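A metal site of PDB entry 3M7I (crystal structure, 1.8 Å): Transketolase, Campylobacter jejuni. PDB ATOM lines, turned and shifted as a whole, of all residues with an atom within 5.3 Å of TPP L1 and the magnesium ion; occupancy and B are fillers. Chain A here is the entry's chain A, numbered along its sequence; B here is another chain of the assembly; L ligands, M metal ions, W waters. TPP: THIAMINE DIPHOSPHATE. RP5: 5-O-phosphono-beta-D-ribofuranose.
OE1 of Glu 394 of chain B sits close to OE2 of Glu 160 (2.5 Å). O of Leu 119 lies within hydrogen-bond range of OH of Tyr 423 of chain B. The side-chain carboxylate (OD1) of Asp 367 of chain B is in hydrogen-bond range of the side-chain hydroxyl (OG) of Ser 188, at 2.6 Å. The backbone NH (N) of Gly 154 is in hydrogen-bond range of the side-chain carboxylate (OD2) of Asp 157. The backbone NH (N) of Ile 189 lies within hydrogen-bond range of the side-chain carboxylate (OD2) of Asp 367 of chain B, at 3.0 Å. The backbone NH of Glu 160 lies close to the backbone carbonyl oxygen of Ile 392 of chain B (3.5 Å).
Of the 30 residues printed, 3 come within 4 Å of the magnesium ion.
Water W3 bridges the backbone carbonyl oxygen (O) of Asp 183 (2.8 Å) and the backbone NH (N) of Asp 155 (3.1 Å). Water W6 lies within hydrogen-bond range of O1A of TPP L1 (2.7 Å), OD2 of Asp 157 (3.0 Å) and N of Gly 154 (3.4 Å). Water W1 lies within hydrogen-bond range of O1B of TPP L1, O of His 259 and N of Ala 34. Water W4 lies within hydrogen-bond range of NE2 of His 456 of chain B (3.4 Å) and N4' of TPP L1 (3.4 Å). Water W2 lies within hydrogen-bond range of OG1 of Thr 416 of chain B, OE2 of Glu 394 of chain B and O of Ala 366 of chain B.
The magnesium ion is bound by water W3 (2.1 Å), O of Ile 187 (2.2 Å), O2A of TPP L1 (2.2 Å), OD1 of Asn 185 (2.2 Å), OD2 of Asp 155 (2.2 Å) and O2B of TPP L1 (2.2 Å).
Merely in contact with TPP L1: Glu 160, Phe 420 of chain B, Tyr 423 of chain B, Asp 367 of chain B, Ala 34, Ile 189, Gly 154, His 456 of chain B, Ser 188, Ile 392 of chain B, Pro 118 and Ile 245. Hydrophobic or aromatic side chains that line TPP L1: Ala 34, His 70, Leu 119, Ile 189, Ile 245, His 259, Ile 392 of chain B, Phe 420 of chain B, Tyr 423 of chain B and His 456 of chain B. Of the 30 residues printed, 21 come within 4 Å of TPP L1.
The side-chain carboxylate (OE2) of Glu 394 of chain B lies within hydrogen-bond range of a nitrogen (N1') of TPP L1. ND1 of His 259 lies within hydrogen-bond range of O3B of TPP L1 (3.1 Å). The backbone NH (N) of Gly 156 is in hydrogen-bond range of an oxygen (O1A) of TPP L1, 2.9 Å away. NE2 of His 70 is in hydrogen-bond range of O1B of TPP L1 (2.9 Å). N4' of TPP L1 is in hydrogen-bond range of O of Gly 117, 2.9 Å away. N3' of TPP L1 sits at hydrogen-bond distance from N of Leu 119 (3.0 Å). A ring nitrogen (NE2) of His 259 sits at hydrogen-bond distance from an oxygen (O2) of RP5 L2, 2.4 Å away. An oxygen (O1A) of TPP L1 lies within hydrogen-bond range of the backbone NH (N) of Asp 155 (3.4 Å).
A sulfur (S1) of TPP L1 sits close to an oxygen (O2) of RP5 L2, 3.5 Å away.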
ATOM      1  N   GLY A  33       6.232 -16.204   9.189  1.00  0.00           N
ATOM      2  CA  GLY A  33       6.960 -15.844   7.963  1.00  0.00           C
ATOM      3  C   GLY A  33       6.745 -16.782   6.828  1.00  0.00           C
ATOM      4  O   GLY A  33       6.428 -16.386   5.716  1.00  0.00           O
ATOM      5  N   ALA A  34       6.997 -18.055   7.076  1.00  0.00           N
ATOM      6  CA  ALA A  34       6.835 -19.071   6.040  1.00  0.00           C
ATOM      7  C   ALA A  34       5.379 -19.192   5.538  1.00  0.00           C
ATOM      8  O   ALA A  34       5.126 -19.205   4.289  1.00  0.00           O
ATOM      9  CB  ALA A  34       7.425 -20.465   6.493  1.00  0.00           C
ATOM     10  N   HIS A  70       7.085 -26.037  10.796  1.00  0.00           N
ATOM     11  CA  HIS A  70       6.847 -24.797  11.462  1.00  0.00           C
ATOM     12  C   HIS A  70       5.847 -23.955  10.724  1.00  0.00           C
ATOM     13  O   HIS A  70       5.340 -22.992  11.311  1.00  0.00           O
ATOM     14  CB  HIS A  70       8.145 -23.964  11.733  1.00  0.00           C
ATOM     15  CG  HIS A  70       8.907 -23.585  10.487  1.00  0.00           C
ATOM     16  ND1 HIS A  70       9.627 -24.522   9.760  1.00  0.00           N
ATOM     17  CD2 HIS A  70       9.020 -22.410   9.821  1.00  0.00           C
ATOM     18  CE1 HIS A  70      10.146 -23.925   8.682  1.00  0.00           C
ATOM     19  NE2 HIS A  70       9.826 -22.637   8.718  1.00  0.00           N
ATOM     20  N   GLY A 117       8.334 -31.347  11.471  1.00  0.00           N
ATOM     21  CA  GLY A 117       8.969 -30.606  12.549  1.00  0.00           C
ATOM     22  C   GLY A 117      10.486 -30.763  12.552  1.00  0.00           C
ATOM     23  O   GLY A 117      11.205 -29.776  12.475  1.00  0.00           O
ATOM     24  N   PRO A 118      10.982 -31.980  12.667  1.00  0.00           N
ATOM     25  CA  PRO A 118      12.433 -32.116  12.496  1.00  0.00           C
ATOM     26  C   PRO A 118      12.752 -31.930  11.002  1.00  0.00           C
ATOM     27  O   PRO A 118      12.232 -32.673  10.189  1.00  0.00           O
ATOM     28  CB  PRO A 118      12.724 -33.556  12.970  1.00  0.00           C
ATOM     29  CG  PRO A 118      11.467 -33.904  13.794  1.00  0.00           C
ATOM     30  CD  PRO A 118      10.349 -33.250  13.022  1.00  0.00           C
ATOM     31  N   LEU A 119      13.573 -30.955  10.689  1.00  0.00           N
ATOM     32  CA  LEU A 119      13.852 -30.585   9.276  1.00  0.00           C
ATOM     33  C   LEU A 119      14.536 -31.680   8.518  1.00  0.00           C
ATOM     34  O   LEU A 119      15.243 -32.536   9.097  1.00  0.00           O
ATOM     35  CB  LEU A 119      14.641 -29.297   9.188  1.00  0.00           C
ATOM     36  CG  LEU A 119      13.972 -27.985   9.639  1.00  0.00           C
ATOM     37  CD1 LEU A 119      15.028 -26.981   9.976  1.00  0.00           C
ATOM     38  CD2 LEU A 119      12.970 -27.409   8.579  1.00  0.00           C
ATOM     39  N   GLY A 154      11.880 -25.898   2.790  1.00  0.00           N
ATOM     40  CA  GLY A 154      12.566 -24.636   2.924  1.00  0.00           C
ATOM     41  C   GLY A 154      14.070 -24.813   2.865  1.00  0.00           C
ATOM     42  O   GLY A 154      14.536 -25.933   2.654  1.00  0.00           O
ATOM     43  N   ASP A 155      14.797 -23.756   3.125  1.00  0.00           N
ATOM     44  CA  ASP A 155      16.257 -23.784   3.155  1.00  0.00           C
ATOM     45  C   ASP A 155      16.767 -24.833   4.128  1.00  0.00           C
ATOM     46  O   ASP A 155      17.758 -25.533   3.884  1.00  0.00           O
ATOM     47  CB  ASP A 155      16.804 -22.429   3.537  1.00  0.00           C
ATOM     48  CG  ASP A 155      16.414 -21.354   2.518  1.00  0.00           C
ATOM     49  OD1 ASP A 155      16.808 -21.521   1.349  1.00  0.00           O
ATOM     50  OD2 ASP A 155      15.698 -20.413   2.849  1.00  0.00           O
ATOM     51  N   GLY A 156      16.072 -24.910   5.246  1.00  0.00           N
ATOM     52  CA  GLY A 156      16.570 -25.777   6.304  1.00  0.00           C
ATOM     53  C   GLY A 156      16.509 -27.210   5.886  1.00  0.00           C
ATOM     54  O   GLY A 156      17.391 -28.028   6.238  1.00  0.00           O
ATOM     55  N   ASP A 157      15.415 -27.575   5.225  1.00  0.00           N
ATOM     56  CA  ASP A 157      15.273 -28.962   4.832  1.00  0.00           C
ATOM     57  C   ASP A 157      16.411 -29.375   3.877  1.00  0.00           C
ATOM     58  O   ASP A 157      16.925 -30.495   3.900  1.00  0.00           O
ATOM     59  CB  ASP A 157      13.951 -29.217   4.109  1.00  0.00           C
ATOM     60  CG  ASP A 157      12.753 -28.958   4.989  1.00  0.00           C
ATOM     61  OD1 ASP A 157      12.537 -29.820   5.880  1.00  0.00           O
ATOM     62  OD2 ASP A 157      12.052 -27.925   4.743  1.00  0.00           O
ATOM     63  N   GLU A 160      19.902 -30.222   5.313  1.00  0.00           N
ATOM     64  CA  GLU A 160      20.042 -31.500   6.079  1.00  0.00           C
ATOM     65  C   GLU A 160      20.487 -32.621   5.135  1.00  0.00           C
ATOM     66  O   GLU A 160      19.932 -32.807   4.022  1.00  0.00           O
ATOM     67  CB  GLU A 160      18.690 -31.858   6.701  1.00  0.00           C
ATOM     68  CG  GLU A 160      18.377 -30.968   7.896  1.00  0.00           C
ATOM     69  CD  GLU A 160      19.204 -31.352   9.137  1.00  0.00           C
ATOM     70  OE1 GLU A 160      20.078 -32.262   9.067  1.00  0.00           O
ATOM     71  OE2 GLU A 160      19.028 -30.700  10.192  1.00  0.00           O
ATOM     72  N   ASP A 183      10.762 -23.472  -1.148  1.00  0.00           N
ATOM     73  CA  ASP A 183      10.566 -22.100  -0.729  1.00  0.00           C
ATOM     74  C   ASP A 183      11.910 -21.384  -0.547  1.00  0.00           C
ATOM     75  O   ASP A 183      12.461 -21.336   0.537  1.00  0.00           O
ATOM     76  CB  ASP A 183       9.795 -22.097   0.610  1.00  0.00           C
ATOM     77  CG  ASP A 183       9.310 -20.740   0.989  1.00  0.00           C
ATOM     78  OD1 ASP A 183       9.245 -19.889   0.081  1.00  0.00           O
ATOM     79  OD2 ASP A 183       8.965 -20.523   2.194  1.00  0.00           O
ATOM     80  N   ASN A 185      13.552 -18.352   0.044  1.00  0.00           N
ATOM     81  CA  ASN A 185      13.374 -16.981   0.552  1.00  0.00           C
ATOM     82  C   ASN A 185      14.655 -16.301   1.099  1.00  0.00           C
ATOM     83  O   ASN A 185      14.637 -15.160   1.592  1.00  0.00           O
ATOM     84  CB  ASN A 185      12.207 -16.965   1.543  1.00  0.00           C
ATOM     85  CG  ASN A 185      12.469 -17.763   2.802  1.00  0.00           C
ATOM     86  OD1 ASN A 185      13.618 -18.205   3.074  1.00  0.00           O
ATOM     87  ND2 ASN A 185      11.389 -17.995   3.566  1.00  0.00           N
ATOM     88  N   ASN A 186      15.768 -17.021   0.996  1.00  0.00           N
ATOM     89  CA  ASN A 186      17.070 -16.576   1.430  1.00  0.00           C
ATOM     90  C   ASN A 186      17.185 -16.174   2.904  1.00  0.00           C
ATOM     91  O   ASN A 186      18.097 -15.496   3.262  1.00  0.00           O
ATOM     92  CB  ASN A 186      17.554 -15.414   0.496  1.00  0.00           C
ATOM     93  CG  ASN A 186      19.013 -15.051   0.709  1.00  0.00           C
ATOM     94  OD1 ASN A 186      19.331 -13.969   1.236  1.00  0.00           O
ATOM     95  ND2 ASN A 186      19.924 -15.948   0.307  1.00  0.00           N
ATOM     96  N   ILE A 187      16.269 -16.681   3.746  1.00  0.00           N
ATOM     97  CA  ILE A 187      16.258 -16.356   5.140  1.00  0.00           C
ATOM     98  C   ILE A 187      16.105 -17.616   5.984  1.00  0.00           C
ATOM     99  O   ILE A 187      15.294 -18.500   5.601  1.00  0.00           O
ATOM    100  CB  ILE A 187      15.091 -15.429   5.437  1.00  0.00           C
ATOM    101  CG1 ILE A 187      15.309 -14.060   4.761  1.00  0.00           C
ATOM    102  CG2 ILE A 187      14.832 -15.319   6.994  1.00  0.00           C
ATOM    103  CD1 ILE A 187      16.360 -13.243   5.352  1.00  0.00           C
ATOM    104  N   SER A 188      16.937 -17.703   7.021  1.00  0.00           N
ATOM    105  CA  SER A 188      16.822 -18.748   8.121  1.00  0.00           C
ATOM    106  C   SER A 188      16.909 -18.030   9.425  1.00  0.00           C
ATOM    107  O   SER A 188      16.815 -16.831   9.465  1.00  0.00           O
ATOM    108  CB  SER A 188      17.902 -19.873   7.932  1.00  0.00           C
ATOM    109  OG  SER A 188      19.189 -19.430   8.254  1.00  0.00           O
ATOM    110  N   ILE A 189      17.074 -18.737  10.551  1.00  0.00           N
ATOM    111  CA  ILE A 189      17.037 -18.087  11.843  1.00  0.00           C
ATOM    112  C   ILE A 189      18.225 -17.145  12.082  1.00  0.00           C
ATOM    113  O   ILE A 189      18.087 -16.064  12.685  1.00  0.00           O
ATOM    114  CB  ILE A 189      16.960 -19.157  12.950  1.00  0.00           C
ATOM    115  CG1 ILE A 189      15.606 -19.892  12.910  1.00  0.00           C
ATOM    116  CG2 ILE A 189      17.225 -18.545  14.309  1.00  0.00           C
ATOM    117  CD1 ILE A 189      15.523 -21.079  13.931  1.00  0.00           C
ATOM    118  N   VAL A 193      20.742 -16.673   4.315  1.00  0.00           N
ATOM    119  CA  VAL A 193      21.120 -18.056   4.039  1.00  0.00           C
ATOM    120  C   VAL A 193      22.535 -18.164   3.410  1.00  0.00           C
ATOM    121  O   VAL A 193      23.251 -19.159   3.639  1.00  0.00           O
ATOM    122  CB  VAL A 193      20.075 -18.670   3.124  1.00  0.00           C
ATOM    123  CG1 VAL A 193      20.577 -19.879   2.393  1.00  0.00           C
ATOM    124  CG2 VAL A 193      18.796 -19.029   3.951  1.00  0.00           C
ATOM    125  N   ILE A 245      10.053 -13.897   2.538  1.00  0.00           N
ATOM    126  CA  ILE A 245       9.546 -14.297   3.839  1.00  0.00           C
ATOM    127  C   ILE A 245       8.602 -13.196   4.353  1.00  0.00           C
ATOM    128  O   ILE A 245       8.866 -12.028   4.203  1.00  0.00           O
ATOM    129  CB  ILE A 245      10.606 -14.732   4.830  1.00  0.00           C
ATOM    130  CG1 ILE A 245       9.963 -15.489   6.003  1.00  0.00           C
ATOM    131  CG2 ILE A 245      11.363 -13.566   5.435  1.00  0.00           C
ATOM    132  CD1 ILE A 245      10.977 -15.925   7.029  1.00  0.00           C
ATOM    133  N   HIS A 259      10.500 -15.065  11.164  1.00  0.00           N
ATOM    134  CA  HIS A 259      10.551 -16.515  11.026  1.00  0.00           C
ATOM    135  C   HIS A 259       9.725 -17.145  12.118  1.00  0.00           C
ATOM    136  O   HIS A 259       8.909 -18.044  11.836  1.00  0.00           O
ATOM    137  CB  HIS A 259      11.991 -17.076  11.119  1.00  0.00           C
ATOM    138  CG  HIS A 259      12.032 -18.521  11.498  1.00  0.00           C
ATOM    139  ND1 HIS A 259      11.844 -19.517  10.583  1.00  0.00           N
ATOM    140  CD2 HIS A 259      12.172 -19.128  12.700  1.00  0.00           C
ATOM    141  CE1 HIS A 259      11.879 -20.697  11.196  1.00  0.00           C
ATOM    142  NE2 HIS A 259      12.068 -20.484  12.485  1.00  0.00           N
ATOM    143  N   ALA B 366      23.929 -24.794  14.757  1.00  0.00           N
ATOM    144  CA  ALA B 366      23.342 -25.229  13.539  1.00  0.00           C
ATOM    145  C   ALA B 366      22.076 -24.380  13.202  1.00  0.00           C
ATOM    146  O   ALA B 366      20.936 -24.850  13.333  1.00  0.00           O
ATOM    147  CB  ALA B 366      23.013 -26.726  13.572  1.00  0.00           C
ATOM    148  N   ASP B 367      22.322 -23.156  12.693  1.00  0.00           N
ATOM    149  CA  ASP B 367      21.301 -22.139  12.411  1.00  0.00           C
ATOM    150  C   ASP B 367      20.536 -21.654  13.624  1.00  0.00           C
ATOM    151  O   ASP B 367      19.531 -21.007  13.427  1.00  0.00           O
ATOM    152  CB  ASP B 367      20.314 -22.591  11.371  1.00  0.00           C
ATOM    153  CG  ASP B 367      19.490 -21.395  10.766  1.00  0.00           C
ATOM    154  OD1 ASP B 367      20.120 -20.333  10.486  1.00  0.00           O
ATOM    155  OD2 ASP B 367      18.251 -21.536  10.667  1.00  0.00           O
ATOM    156  N   LEU B 368      20.942 -22.007  14.852  1.00  0.00           N
ATOM    157  CA  LEU B 368      20.142 -21.634  16.051  1.00  0.00           C
ATOM    158  C   LEU B 368      20.815 -20.658  17.036  1.00  0.00           C
ATOM    159  O   LEU B 368      20.394 -20.507  18.249  1.00  0.00           O
ATOM    160  CB  LEU B 368      19.669 -22.904  16.786  1.00  0.00           C
ATOM    161  CG  LEU B 368      18.590 -23.671  16.058  1.00  0.00           C
ATOM    162  CD1 LEU B 368      18.325 -25.007  16.792  1.00  0.00           C
ATOM    163  CD2 LEU B 368      17.324 -22.783  16.025  1.00  0.00           C
ATOM    164  N   ILE B 392      21.901 -25.638   8.777  1.00  0.00           N
ATOM    165  CA  ILE B 392      21.047 -26.697   9.291  1.00  0.00           C
ATOM    166  C   ILE B 392      21.698 -28.082   9.014  1.00  0.00           C
ATOM    167  O   ILE B 392      21.199 -28.890   8.235  1.00  0.00           O
ATOM    168  CB  ILE B 392      19.589 -26.609   8.831  1.00  0.00           C
ATOM    169  CG1 ILE B 392      19.016 -25.184   9.144  1.00  0.00           C
ATOM    170  CG2 ILE B 392      18.776 -27.656   9.635  1.00  0.00           C
ATOM    171  CD1 ILE B 392      19.284 -24.074   8.211  1.00  0.00           C
ATOM    172  N   GLU B 394      23.493 -30.416  11.676  1.00  0.00           N
ATOM    173  CA  GLU B 394      23.945 -30.765  13.009  1.00  0.00           C
ATOM    174  C   GLU B 394      25.032 -31.827  12.940  1.00  0.00           C
ATOM    175  O   GLU B 394      26.038 -31.721  13.613  1.00  0.00           O
ATOM    176  CB  GLU B 394      22.813 -31.404  13.812  1.00  0.00           C
ATOM    177  CG  GLU B 394      21.718 -30.471  14.177  1.00  0.00           C
ATOM    178  CD  GLU B 394      20.686 -30.298  13.085  1.00  0.00           C
ATOM    179  OE1 GLU B 394      20.679 -31.039  12.076  1.00  0.00           O
ATOM    180  OE2 GLU B 394      19.827 -29.385  13.265  1.00  0.00           O
ATOM    181  N   THR B 416      22.961 -26.882  19.300  1.00  0.00           N
ATOM    182  CA  THR B 416      21.627 -27.079  18.768  1.00  0.00           C
ATOM    183  C   THR B 416      20.612 -27.282  19.951  1.00  0.00           C
ATOM    184  O   THR B 416      21.041 -27.248  21.107  1.00  0.00           O
ATOM    185  CB  THR B 416      21.556 -28.228  17.742  1.00  0.00           C
ATOM    186  OG1 THR B 416      20.288 -28.228  17.109  1.00  0.00           O
ATOM    187  CG2 THR B 416      21.989 -29.605  18.390  1.00  0.00           C
ATOM    188  N   PHE B 417      19.333 -27.481  19.600  1.00  0.00           N
ATOM    189  CA  PHE B 417      18.294 -27.886  20.577  1.00  0.00           C
ATOM    190  C   PHE B 417      18.610 -29.324  21.013  1.00  0.00           C
ATOM    191  O   PHE B 417      19.092 -30.162  20.230  1.00  0.00           O
ATOM    192  CB  PHE B 417      16.881 -27.869  20.046  1.00  0.00           C
ATOM    193  CG  PHE B 417      16.350 -26.512  19.664  1.00  0.00           C
ATOM    194  CD1 PHE B 417      16.806 -25.369  20.310  1.00  0.00           C
ATOM    195  CD2 PHE B 417      15.404 -26.424  18.717  1.00  0.00           C
ATOM    196  CE1 PHE B 417      16.266 -24.132  19.937  1.00  0.00           C
ATOM    197  CE2 PHE B 417      14.867 -25.144  18.339  1.00  0.00           C
ATOM    198  CZ  PHE B 417      15.299 -24.065  18.990  1.00  0.00           C
ATOM    199  N   PHE B 420      17.543 -32.141  18.840  1.00  0.00           N
ATOM    200  CA  PHE B 420      18.311 -32.414  17.629  1.00  0.00           C
ATOM    201  C   PHE B 420      19.764 -32.838  17.902  1.00  0.00           C
ATOM    202  O   PHE B 420      20.531 -33.023  16.949  1.00  0.00           O
ATOM    203  CB  PHE B 420      18.172 -31.225  16.670  1.00  0.00           C
ATOM    204  CG  PHE B 420      16.738 -30.858  16.378  1.00  0.00           C
ATOM    205  CD1 PHE B 420      15.838 -31.779  16.043  1.00  0.00           C
ATOM    206  CD2 PHE B 420      16.312 -29.543  16.461  1.00  0.00           C
ATOM    207  CE1 PHE B 420      14.437 -31.457  15.784  1.00  0.00           C
ATOM    208  CE2 PHE B 420      14.961 -29.205  16.216  1.00  0.00           C
ATOM    209  CZ  PHE B 420      14.046 -30.173  15.893  1.00  0.00           C
ATOM    210  N   TYR B 423      20.422 -35.921  15.791  1.00  0.00           N
ATOM    211  CA  TYR B 423      20.978 -35.842  14.437  1.00  0.00           C
ATOM    212  C   TYR B 423      22.521 -35.940  14.423  1.00  0.00           C
ATOM    213  O   TYR B 423      23.074 -36.242  13.360  1.00  0.00           O
ATOM    214  CB  TYR B 423      20.547 -34.551  13.736  1.00  0.00           C
ATOM    215  CG  TYR B 423      19.213 -34.504  13.088  1.00  0.00           C
ATOM    216  CD1 TYR B 423      18.008 -34.550  13.813  1.00  0.00           C
ATOM    217  CD2 TYR B 423      19.107 -34.227  11.709  1.00  0.00           C
ATOM    218  CE1 TYR B 423      16.800 -34.517  13.202  1.00  0.00           C
ATOM    219  CE2 TYR B 423      17.889 -34.184  11.099  1.00  0.00           C
ATOM    220  CZ  TYR B 423      16.742 -34.247  11.839  1.00  0.00           C
ATOM    221  OH  TYR B 423      15.540 -34.144  11.210  1.00  0.00           O
ATOM    222  N   HIS B 456       9.623 -31.356  19.423  1.00  0.00           N
ATOM    223  CA  HIS B 456      10.635 -30.495  19.949  1.00  0.00           C
ATOM    224  C   HIS B 456      10.882 -30.641  21.462  1.00  0.00           C
ATOM    225  O   HIS B 456      11.637 -29.840  21.989  1.00  0.00           O
ATOM    226  CB  HIS B 456      10.294 -29.024  19.628  1.00  0.00           C
ATOM    227  CG  HIS B 456      10.499 -28.664  18.157  1.00  0.00           C
ATOM    228  ND1 HIS B 456      11.251 -27.574  17.735  1.00  0.00           N
ATOM    229  CD2 HIS B 456      10.010 -29.235  17.046  1.00  0.00           C
ATOM    230  CE1 HIS B 456      11.235 -27.538  16.402  1.00  0.00           C
ATOM    231  NE2 HIS B 456      10.477 -28.518  15.960  1.00  0.00           N
HETATM  232  N1' TPP L   1      17.165 -28.725  13.141  1.00  0.00           N
HETATM  233  C2' TPP L   1      16.261 -29.589  12.707  1.00  0.00           C
HETATM  234  CM2 TPP L   1      16.634 -30.979  12.245  1.00  0.00           C
HETATM  235  N3' TPP L   1      14.977 -29.251  12.784  1.00  0.00           N
HETATM  236  C4' TPP L   1      14.549 -28.086  13.253  1.00  0.00           C
HETATM  237  N4' TPP L   1      13.236 -27.862  13.263  1.00  0.00           N
HETATM  238  C5' TPP L   1      15.535 -27.087  13.663  1.00  0.00           C
HETATM  239  C6' TPP L   1      16.834 -27.511  13.589  1.00  0.00           C
HETATM  240  C7' TPP L   1      15.180 -25.725  14.203  1.00  0.00           C
HETATM  241  N3  TPP L   1      14.571 -24.914  13.184  1.00  0.00           N
HETATM  242  C2  TPP L   1      13.274 -24.669  13.021  1.00  0.00           C
HETATM  243  S1  TPP L   1      12.883 -23.756  11.567  1.00  0.00           S
HETATM  244  C5  TPP L   1      14.599 -23.613  11.292  1.00  0.00           C
HETATM  245  C4  TPP L   1      15.334 -24.344  12.232  1.00  0.00           C
HETATM  246  CM4 TPP L   1      16.844 -24.377  12.128  1.00  0.00           C
HETATM  247  C6  TPP L   1      15.235 -22.873  10.166  1.00  0.00           C
HETATM  248  C7  TPP L   1      14.212 -22.409   9.212  1.00  0.00           C
HETATM  249  O7  TPP L   1      14.897 -22.149   8.029  1.00  0.00           O
HETATM  250  PA  TPP L   1      14.016 -22.221   6.755  1.00  0.00           P
HETATM  251  O1A TPP L   1      13.711 -23.627   6.361  1.00  0.00           O
HETATM  252  O2A TPP L   1      14.807 -21.436   5.767  1.00  0.00           O
HETATM  253  O3A TPP L   1      12.597 -21.610   7.199  1.00  0.00           O
HETATM  254  PB  TPP L   1      12.105 -20.095   6.967  1.00  0.00           P
HETATM  255  O1B TPP L   1      10.769 -20.078   7.640  1.00  0.00           O
HETATM  256  O2B TPP L   1      12.238 -19.819   5.465  1.00  0.00           O
HETATM  257  O3B TPP L   1      13.017 -19.229   7.779  1.00  0.00           O
HETATM  258  C1  RP5 L   2      11.628 -23.107  16.339  1.00  0.00           C
HETATM  259  O4  RP5 L   2      12.390 -22.803  17.474  1.00  0.00           O
HETATM  260  C2  RP5 L   2      11.468 -21.793  15.593  1.00  0.00           C
HETATM  261  O2  RP5 L   2      12.316 -21.854  14.471  1.00  0.00           O
HETATM  262  C3  RP5 L   2      11.728 -20.696  16.610  1.00  0.00           C
HETATM  263  O3  RP5 L   2      12.487 -19.602  16.147  1.00  0.00           O
HETATM  264  C4  RP5 L   2      12.520 -21.424  17.657  1.00  0.00           C
HETATM  265  C5  RP5 L   2      11.978 -21.102  19.019  1.00  0.00           C
HETATM  266  O5  RP5 L   2      12.459 -19.799  19.339  1.00  0.00           O
HETATM  267  P'  RP5 L   2      12.775 -19.620  20.862  1.00  0.00           P
HETATM  268  O1X RP5 L   2      14.154 -19.099  21.142  1.00  0.00           O
HETATM  269  O2X RP5 L   2      12.469 -21.102  21.473  1.00  0.00           O
HETATM  270  O3X RP5 L   2      11.858 -18.500  21.559  1.00  0.00           O
HETATM  271  O1  RP5 L   2      10.343 -23.551  16.726  1.00  0.00           O
HETATM  272 MG    MG M   1      14.187 -19.887   4.355  1.00  0.00          MG
HETATM  273  O   HOH W   1       8.773 -19.017   9.239  1.00  0.00           O
HETATM  274  O   HOH W   2      19.936 -27.226  14.758  1.00  0.00           O
HETATM  275  O   HOH W   3      12.946 -21.224   3.299  1.00  0.00           O
HETATM  276  O   HOH W   4      10.436 -26.006  13.719  1.00  0.00           O
HETATM  277  O   HOH W   5      10.230 -21.589   4.130  1.00  0.00           O
HETATM  278  O   HOH W   6      11.574 -25.311   6.144  1.00  0.00           O
